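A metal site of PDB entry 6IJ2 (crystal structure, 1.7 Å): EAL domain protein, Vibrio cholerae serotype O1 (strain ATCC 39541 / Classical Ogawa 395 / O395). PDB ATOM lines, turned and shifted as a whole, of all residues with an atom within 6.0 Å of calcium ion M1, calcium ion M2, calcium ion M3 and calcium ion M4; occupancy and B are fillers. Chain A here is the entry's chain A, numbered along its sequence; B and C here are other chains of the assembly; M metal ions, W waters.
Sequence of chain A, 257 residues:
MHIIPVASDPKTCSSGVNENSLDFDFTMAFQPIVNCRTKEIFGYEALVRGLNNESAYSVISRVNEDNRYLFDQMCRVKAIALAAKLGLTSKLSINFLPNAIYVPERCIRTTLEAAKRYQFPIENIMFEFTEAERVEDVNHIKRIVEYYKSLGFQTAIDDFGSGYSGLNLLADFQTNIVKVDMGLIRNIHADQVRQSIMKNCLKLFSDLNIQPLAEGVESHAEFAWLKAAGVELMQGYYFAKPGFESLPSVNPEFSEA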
ATOM      1  N   GLU A  45      -2.637  15.871  16.257  1.00  0.00           N
ATOM      2  CA  GLU A  45      -3.454  14.682  16.344  1.00  0.00           C
ATOM      3  C   GLU A  45      -4.864  15.088  16.776  1.00  0.00           C
ATOM      4  O   GLU A  45      -5.023  15.879  17.723  1.00  0.00           O
ATOM      5  CB  GLU A  45      -2.867  13.666  17.324  1.00  0.00           C
ATOM      6  CG  GLU A  45      -3.727  12.434  17.432  1.00  0.00           C
ATOM      7  CD  GLU A  45      -3.201  11.395  18.396  1.00  0.00           C
ATOM      8  OE1 GLU A  45      -2.242  11.674  19.156  1.00  0.00           O
ATOM      9  OE2 GLU A  45      -3.777  10.286  18.372  1.00  0.00           O
ATOM     10  N   LEU A  47      -8.381  14.214  18.462  1.00  0.00           N
ATOM     11  CA  LEU A  47      -8.774  13.349  19.571  1.00  0.00           C
ATOM     12  C   LEU A  47     -10.233  13.602  19.906  1.00  0.00           C
ATOM     13  O   LEU A  47     -10.632  14.756  20.100  1.00  0.00           O
ATOM     14  CB  LEU A  47      -7.911  13.605  20.798  1.00  0.00           C
ATOM     15  CG  LEU A  47      -6.420  13.317  20.597  1.00  0.00           C
ATOM     16  CD1 LEU A  47      -5.640  14.024  21.677  1.00  0.00           C
ATOM     17  CD2 LEU A  47      -6.157  11.811  20.643  1.00  0.00           C
ATOM     18  N   ASN A  95      -6.848   9.008  14.300  1.00  0.00           N
ATOM     19  CA  ASN A  95      -6.766   7.651  14.831  1.00  0.00           C
ATOM     20  C   ASN A  95      -7.720   6.751  14.051  1.00  0.00           C
ATOM     21  O   ASN A  95      -8.899   7.074  13.884  1.00  0.00           O
ATOM     22  CB  ASN A  95      -7.140   7.637  16.312  1.00  0.00           C
ATOM     23  CG  ASN A  95      -6.077   8.264  17.184  1.00  0.00           C
ATOM     24  OD1 ASN A  95      -5.055   7.655  17.482  1.00  0.00           O
ATOM     25  ND2 ASN A  95      -6.312   9.506  17.599  1.00  0.00           N
ATOM     26  N   GLU A 128      -3.283   7.004  11.974  1.00  0.00           N
ATOM     27  CA  GLU A 128      -2.555   6.251  12.989  1.00  0.00           C
ATOM     28  C   GLU A 128      -3.256   4.916  13.223  1.00  0.00           C
ATOM     29  O   GLU A 128      -4.464   4.883  13.489  1.00  0.00           O
ATOM     30  CB  GLU A 128      -2.461   7.035  14.294  1.00  0.00           C
ATOM     31  CG  GLU A 128      -1.936   8.440  14.083  1.00  0.00           C
ATOM     32  CD  GLU A 128      -1.699   9.179  15.374  1.00  0.00           C
ATOM     33  OE1 GLU A 128      -1.209  10.319  15.307  1.00  0.00           O
ATOM     34  OE2 GLU A 128      -1.982   8.620  16.465  1.00  0.00           O
ATOM     35  N   THR A 130      -3.844   1.336  15.074  1.00  0.00           N
ATOM     36  CA  THR A 130      -3.803   0.497  16.259  1.00  0.00           C
ATOM     37  C   THR A 130      -4.512  -0.816  15.934  1.00  0.00           C
ATOM     38  O   THR A 130      -5.581  -0.823  15.306  1.00  0.00           O
ATOM     39  CB  THR A 130      -4.503   1.154  17.462  1.00  0.00           C
ATOM     40  OG1 THR A 130      -3.884   2.414  17.757  1.00  0.00           O
ATOM     41  CG2 THR A 130      -4.410   0.254  18.688  1.00  0.00           C
ATOM     42  N   GLU A 131      -3.921  -1.918  16.370  1.00  0.00           N
ATOM     43  CA  GLU A 131      -4.504  -3.238  16.140  1.00  0.00           C
ATOM     44  C   GLU A 131      -5.719  -3.458  17.036  1.00  0.00           C
ATOM     45  O   GLU A 131      -5.772  -2.972  18.172  1.00  0.00           O
ATOM     46  CB  GLU A 131      -3.463  -4.320  16.396  1.00  0.00           C
ATOM     47  CG  GLU A 131      -2.109  -4.058  15.731  1.00  0.00           C
ATOM     48  CD  GLU A 131      -1.122  -3.321  16.640  1.00  0.00           C
ATOM     49  OE1 GLU A 131      -1.515  -2.293  17.233  1.00  0.00           O
ATOM     50  OE2 GLU A 131       0.033  -3.782  16.759  1.00  0.00           O
ATOM     51  N   ILE A 157       2.284   3.768  12.666  1.00  0.00           N
ATOM     52  CA  ILE A 157       1.984   2.810  13.725  1.00  0.00           C
ATOM     53  C   ILE A 157       1.853   3.594  15.021  1.00  0.00           C
ATOM     54  O   ILE A 157       2.763   4.310  15.431  1.00  0.00           O
ATOM     55  CB  ILE A 157       3.075   1.723  13.820  1.00  0.00           C
ATOM     56  CG1 ILE A 157       3.063   0.881  12.551  1.00  0.00           C
ATOM     57  CG2 ILE A 157       2.851   0.856  15.056  1.00  0.00           C
ATOM     58  CD1 ILE A 157       4.121  -0.157  12.514  1.00  0.00           C
ATOM     59  N   ASP A 158       0.684   3.486  15.660  1.00  0.00           N
ATOM     60  CA  ASP A 158       0.360   4.355  16.797  1.00  0.00           C
ATOM     61  C   ASP A 158       1.047   3.904  18.090  1.00  0.00           C
ATOM     62  O   ASP A 158       1.541   4.728  18.870  1.00  0.00           O
ATOM     63  CB  ASP A 158      -1.161   4.374  16.959  1.00  0.00           C
ATOM     64  CG  ASP A 158      -1.678   5.512  17.828  1.00  0.00           C
ATOM     65  OD1 ASP A 158      -0.884   6.255  18.448  1.00  0.00           O
ATOM     66  OD2 ASP A 158      -2.907   5.683  17.861  1.00  0.00           O
ATOM     67  N   ASP A 159       1.095   2.619  18.349  1.00  0.00           N
ATOM     68  CA  ASP A 159       1.362   2.218  19.721  1.00  0.00           C
ATOM     69  C   ASP A 159       2.562   1.299  19.761  1.00  0.00           C
ATOM     70  O   ASP A 159       2.490   0.206  20.322  1.00  0.00           O
ATOM     71  CB  ASP A 159       0.144   1.547  20.350  1.00  0.00           C
ATOM     72  CG  ASP A 159      -1.111   2.438  20.322  1.00  0.00           C
ATOM     73  OD1 ASP A 159      -1.002   3.665  20.131  1.00  0.00           O
ATOM     74  OD2 ASP A 159      -2.226   1.884  20.526  1.00  0.00           O
ATOM     75  N   PHE A 160       3.680   1.716  19.186  1.00  0.00           N
ATOM     76  CA  PHE A 160       4.886   0.890  19.269  1.00  0.00           C
ATOM     77  C   PHE A 160       5.410   0.857  20.705  1.00  0.00           C
ATOM     78  O   PHE A 160       5.678   1.887  21.313  1.00  0.00           O
ATOM     79  CB  PHE A 160       5.966   1.414  18.348  1.00  0.00           C
ATOM     80  CG  PHE A 160       7.156   0.510  18.254  1.00  0.00           C
ATOM     81  CD1 PHE A 160       7.195  -0.499  17.313  1.00  0.00           C
ATOM     82  CD2 PHE A 160       8.230   0.674  19.102  1.00  0.00           C
ATOM     83  CE1 PHE A 160       8.295  -1.329  17.209  1.00  0.00           C
ATOM     84  CE2 PHE A 160       9.334  -0.160  19.025  1.00  0.00           C
ATOM     85  CZ  PHE A 160       9.360  -1.154  18.073  1.00  0.00           C
ATOM     86  N   GLY A 161       5.607  -0.339  21.223  1.00  0.00           N
ATOM     87  CA  GLY A 161       6.090  -0.491  22.573  1.00  0.00           C
ATOM     88  C   GLY A 161       5.026  -0.683  23.624  1.00  0.00           C
ATOM     89  O   GLY A 161       5.364  -0.703  24.815  1.00  0.00           O
ATOM     90  N   SER A 162       3.770  -0.830  23.235  1.00  0.00           N
ATOM     91  CA  SER A 162       2.717  -1.209  24.160  1.00  0.00           C
ATOM     92  C   SER A 162       1.685  -2.060  23.436  1.00  0.00           C
ATOM     93  O   SER A 162       1.735  -2.208  22.218  1.00  0.00           O
ATOM     94  CB  SER A 162       2.032   0.019  24.765  1.00  0.00           C
ATOM     95  OG  SER A 162       1.339   0.717  23.750  1.00  0.00           O
ATOM     96  N   GLY A 163       0.745  -2.607  24.180  1.00  0.00           N
ATOM     97  CA  GLY A 163      -0.350  -3.312  23.540  1.00  0.00           C
ATOM     98  C   GLY A 163       0.105  -4.531  22.748  1.00  0.00           C
ATOM     99  O   GLY A 163       0.745  -5.448  23.293  1.00  0.00           O
ATOM    100  N   TYR A 164      -0.211  -4.551  21.460  1.00  0.00           N
ATOM    101  CA  TYR A 164       0.156  -5.637  20.565  1.00  0.00           C
ATOM    102  C   TYR A 164       1.545  -5.408  19.985  1.00  0.00           C
ATOM    103  O   TYR A 164       2.069  -4.301  20.001  1.00  0.00           O
ATOM    104  CB  TYR A 164      -0.903  -5.773  19.474  1.00  0.00           C
ATOM    105  CG  TYR A 164      -2.273  -6.069  20.077  1.00  0.00           C
ATOM    106  CD1 TYR A 164      -2.547  -7.309  20.610  1.00  0.00           C
ATOM    107  CD2 TYR A 164      -3.261  -5.087  20.138  1.00  0.00           C
ATOM    108  CE1 TYR A 164      -3.780  -7.595  21.172  1.00  0.00           C
ATOM    109  CE2 TYR A 164      -4.506  -5.367  20.696  1.00  0.00           C
ATOM    110  CZ  TYR A 164      -4.760  -6.618  21.223  1.00  0.00           C
ATOM    111  OH  TYR A 164      -5.984  -6.910  21.776  1.00  0.00           O
ATOM    112  N   SER A 165       2.156  -6.485  19.474  1.00  0.00           N
ATOM    113  CA  SER A 165       3.552  -6.432  19.045  1.00  0.00           C
ATOM    114  C   SER A 165       3.704  -5.550  17.815  1.00  0.00           C
ATOM    115  O   SER A 165       3.204  -5.891  16.736  1.00  0.00           O
ATOM    116  CB  SER A 165       4.084  -7.839  18.754  1.00  0.00           C
ATOM    117  OG  SER A 165       5.382  -7.757  18.149  1.00  0.00           O
ATOM    118  N   GLY A 166       4.410  -4.426  17.981  1.00  0.00           N
ATOM    119  CA  GLY A 166       4.710  -3.571  16.848  1.00  0.00           C
ATOM    120  C   GLY A 166       5.764  -4.143  15.930  1.00  0.00           C
ATOM    121  O   GLY A 166       5.748  -3.890  14.734  1.00  0.00           O
ATOM    122  N   LYS A 179       5.016   5.830  15.996  1.00  0.00           N
ATOM    123  CA  LYS A 179       4.863   6.563  17.244  1.00  0.00           C
ATOM    124  C   LYS A 179       5.252   5.646  18.400  1.00  0.00           C
ATOM    125  O   LYS A 179       4.754   4.523  18.492  1.00  0.00           O
ATOM    126  CB  LYS A 179       3.422   7.045  17.425  1.00  0.00           C
ATOM    127  CG  LYS A 179       3.034   7.999  16.303  1.00  0.00           C
ATOM    128  CD  LYS A 179       2.451   9.321  16.820  1.00  0.00           C
ATOM    129  CE  LYS A 179       1.044   9.191  17.195  1.00  0.00           C
ATOM    130  NZ  LYS A 179       0.408  10.497  17.616  1.00  0.00           N
ATOM    131  N   VAL A 180       6.136   6.124  19.268  1.00  0.00           N
ATOM    132  CA  VAL A 180       6.659   5.300  20.360  1.00  0.00           C
ATOM    133  C   VAL A 180       5.867   5.612  21.610  1.00  0.00           C
ATOM    134  O   VAL A 180       5.820   6.760  22.068  1.00  0.00           O
ATOM    135  CB  VAL A 180       8.167   5.537  20.581  1.00  0.00           C
ATOM    136  CG1 VAL A 180       8.656   4.674  21.767  1.00  0.00           C
ATOM    137  CG2 VAL A 180       8.930   5.189  19.323  1.00  0.00           C
ATOM    138  N   ASP A 181       5.290   4.555  22.203  1.00  0.00           N
ATOM    139  CA  ASP A 181       4.410   4.691  23.351  1.00  0.00           C
ATOM    140  C   ASP A 181       5.128   5.396  24.498  1.00  0.00           C
ATOM    141  O   ASP A 181       6.315   5.192  24.726  1.00  0.00           O
ATOM    142  CB  ASP A 181       3.935   3.314  23.798  1.00  0.00           C
ATOM    143  CG  ASP A 181       2.983   3.391  24.969  1.00  0.00           C
ATOM    144  OD1 ASP A 181       1.814   3.745  24.754  1.00  0.00           O
ATOM    145  OD2 ASP A 181       3.400   3.098  26.104  1.00  0.00           O
ATOM    146  N   GLU A 215       5.907   9.777  21.869  1.00  0.00           N
ATOM    147  CA  GLU A 215       4.641  10.139  22.496  1.00  0.00           C
ATOM    148  C   GLU A 215       4.783  10.376  23.997  1.00  0.00           C
ATOM    149  O   GLU A 215       5.614   9.760  24.670  1.00  0.00           O
ATOM    150  CB  GLU A 215       3.579   9.062  22.284  1.00  0.00           C
ATOM    151  CG  GLU A 215       3.197   8.770  20.840  1.00  0.00           C
ATOM    152  CD  GLU A 215       2.063   7.756  20.735  1.00  0.00           C
ATOM    153  OE1 GLU A 215       1.160   7.966  19.915  1.00  0.00           O
ATOM    154  OE2 GLU A 215       2.050   6.743  21.481  1.00  0.00           O
ATOM    155  OP3   G B   1      -1.617   6.824  21.633  1.00  0.00           O
ATOM    156  P     G B   1      -3.040   6.918  21.822  1.00  0.00           P
ATOM    157  OP1   G B   1      -3.669   7.544  20.707  1.00  0.00           O
ATOM    158  OP2   G B   1      -3.465   5.599  22.162  1.00  0.00           O
ATOM    159  O5'   G B   1      -3.161   7.803  23.118  1.00  0.00           O
ATOM    160  C5'   G B   1      -3.565   9.166  23.049  1.00  0.00           C
ATOM    161  C4'   G B   1      -3.920   9.659  24.434  1.00  0.00           C
ATOM    162  O4'   G B   1      -2.725  10.107  25.106  1.00  0.00           O
ATOM    163  C3'   G B   1      -4.885  10.842  24.509  1.00  0.00           C
ATOM    164  O3'   G B   1      -5.936  10.650  25.436  1.00  0.00           O
ATOM    165  C2'   G B   1      -4.016  11.988  24.994  1.00  0.00           C
ATOM    166  O2'   G B   1      -4.644  12.931  25.812  1.00  0.00           O
ATOM    167  C1'   G B   1      -3.006  11.239  25.850  1.00  0.00           C
ATOM    168  N9    G B   1      -1.772  11.985  26.056  1.00  0.00           N
ATOM    169  C8    G B   1      -1.156  12.824  25.147  1.00  0.00           C
ATOM    170  N7    G B   1      -0.048  13.338  25.603  1.00  0.00           N
ATOM    171  C5    G B   1       0.077  12.800  26.874  1.00  0.00           C
ATOM    172  C6    G B   1       1.085  12.994  27.852  1.00  0.00           C
ATOM    173  O6    G B   1       2.084  13.695  27.797  1.00  0.00           O
ATOM    174  N1    G B   1       0.826  12.275  29.008  1.00  0.00           N
ATOM    175  C2    G B   1      -0.267  11.460  29.190  1.00  0.00           C
ATOM    176  N2    G B   1      -0.330  10.824  30.358  1.00  0.00           N
ATOM    177  N3    G B   1      -1.203  11.258  28.286  1.00  0.00           N
ATOM    178  C4    G B   1      -0.969  11.956  27.160  1.00  0.00           C
ATOM    179  P     G B   2      -7.388  10.797  25.007  1.00  0.00           P
ATOM    180  OP1   G B   2      -7.473  11.937  24.151  1.00  0.00           O
ATOM    181  OP2   G B   2      -8.173  10.746  26.197  1.00  0.00           O
ATOM    182  O5'   G B   2      -7.679   9.485  24.183  1.00  0.00           O
ATOM    183  C5'   G B   2      -7.958   8.248  24.825  1.00  0.00           C
ATOM    184  C4'   G B   2      -7.992   7.140  23.800  1.00  0.00           C
ATOM    185  O4'   G B   2      -8.998   7.437  22.812  1.00  0.00           O
ATOM    186  C3'   G B   2      -6.689   6.929  23.024  1.00  0.00           C
ATOM    187  O3'   G B   2      -6.384   5.553  22.874  1.00  0.00           O
ATOM    188  C2'   G B   2      -7.013   7.486  21.642  1.00  0.00           C
ATOM    189  O2'   G B   2      -6.322   6.899  20.574  1.00  0.00           O
ATOM    190  C1'   G B   2      -8.498   7.179  21.544  1.00  0.00           C
ATOM    191  N9    G B   2      -9.140   8.084  20.599  1.00  0.00           N
ATOM    192  C8    G B   2      -9.227   9.442  20.698  1.00  0.00           C
ATOM    193  N7    G B   2      -9.796   9.992  19.670  1.00  0.00           N
ATOM    194  C5    G B   2     -10.083   8.928  18.828  1.00  0.00           C
ATOM    195  C6    G B   2     -10.700   8.905  17.564  1.00  0.00           C
ATOM    196  O6    G B   2     -11.107   9.846  16.885  1.00  0.00           O
ATOM    197  N1    G B   2     -10.796   7.616  17.069  1.00  0.00           N
ATOM    198  C2    G B   2     -10.347   6.490  17.705  1.00  0.00           C
ATOM    199  N2    G B   2     -10.527   5.342  17.064  1.00  0.00           N
ATOM    200  N3    G B   2      -9.789   6.500  18.896  1.00  0.00           N
ATOM    201  C4    G B   2      -9.688   7.745  19.397  1.00  0.00           C
ATOM    202  N   SER C 165       3.106  -6.966  22.959  1.00  0.00           N
ATOM    203  CA  SER C 165       4.387  -6.265  22.811  1.00  0.00           C
ATOM    204  C   SER C 165       5.435  -6.814  23.780  1.00  0.00           C
ATOM    205  O   SER C 165       5.311  -6.648  24.991  1.00  0.00           O
ATOM    206  CB  SER C 165       4.190  -4.762  23.022  1.00  0.00           C
ATOM    207  OG  SER C 165       5.444  -4.074  23.107  1.00  0.00           O
HETATM  208 CA    CA M   1       1.774  -2.092  19.993  1.00  0.00          CA
HETATM  209 CA    CA M   2       0.150   5.795  20.490  1.00  0.00          CA
HETATM  210 CA    CA M   3      -2.921   8.034  18.448  1.00  0.00          CA
HETATM  211 CA    CA M   4      -3.800   3.753  20.195  1.00  0.00          CA
HETATM  212  O   HOH W   1       0.455   4.307  22.263  1.00  0.00           O
HETATM  213  O   HOH W   2      -0.728  -2.106  19.851  1.00  0.00           O
HETATM  214  O   HOH W   3       1.859  -1.819  17.626  1.00  0.00           O
HETATM  215  O   HOH W   4      -6.191   3.776  20.302  1.00  0.00           O
HETATM  216  O   HOH W   5      -1.301   9.166  19.670  1.00  0.00           O
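The side-chain carboxylate of Asp 181 sits at hydrogen-bond distance from the side-chain hydroxyl of Ser 162 (3.2 Å).
The side-chain carboxylate (OE1) of Glu 128 lies within salt-bridge range of the side-chain amino group (NZ) of Lys 179 (2.8 Å).
The side-chain amino group (NZ) of Lys 179 sits close to the side-chain carboxylate (OE1) of Glu 215, 3.5 Å away.
The backbone NH (N) of Glu 215 lies within hydrogen-bond range of the backbone carbonyl oxygen (O) of Val 180 (3.0 Å).
OD1 of Asn 95 lies close to O2' of G 2 of chain B, 3.4 Å away.
The side-chain amino group of Lys 179 is in salt-bridge range of the side-chain carboxylate of Glu 45.
Three residues have an atom within 4 Å of calcium ion M1: Asp 159, Ser 162 and Tyr 164.
Along chain A the residues within 4 Å of calcium ion M1 span positions 159 to 164.
Water W2 bridges the side-chain carboxylate (OE1) of Glu 131 and the backbone NH (N) of Tyr 164.
Water W5 lies within hydrogen-bond range of OE1 of Glu 45 (2.7 Å) and NZ of Lys 179 (3.0 Å).
Of the 23 residues printed, 4 come within 4 Å of calcium ion M4.
Calcium ion M4 is bound by water W4, OD2 of Asp 159, OP2 of G 1 of chain B, OG1 of Thr 130 and OD1 of Asp 159.
Five residues have an atom within 4 Å of calcium ion M3: Glu 45, Asn 95, Glu 128, Asp 158 and G 1 of chain B.
Along chain A the residues within 4 Å of calcium ion M3 span positions 45 to 158.
Calcium ion M3 is bound by OE2 of Glu 128 (2.3 Å), water W5 (2.3 Å), OD1 of Asn 95 (2.4 Å), OE2 of Glu 45 (2.4 Å), OD2 of Asp 158 (2.4 Å), OP1 of G 1 of chain B (2.4 Å) and OD1 of Asp 158 (2.7 Å).
Four residues have an atom within 4 Å of calcium ion M2: Asp 158, Asp 159, Glu 215 and G 1 of chain B.
The nearest printed residue that does not touch calcium ion M2 is Lys 179 (4.7 Å).
Calcium ion M1 is bound by the backbone carbonyl oxygen of Ser 162 (2.2 Å), the backbone carbonyl oxygen of Tyr 164 (2.2 Å), water W3 (2.4 Å), the backbone carbonyl oxygen of Asp 159 (2.4 Å) and water W2 (2.5 Å).
Calcium ion M1 has five donor atoms within binding distance.
Calcium ion M2 is bound by water W1 (2.3 Å), OD1 of Asp 158 (2.3 Å), OP3 of G 1 of chain B (2.3 Å), OE2 of Glu 215 (2.3 Å), O of Asp 158 (2.4 Å), OD1 of Asp 159 (2.4 Å) and OE1 of Glu 215 (2.5 Å).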
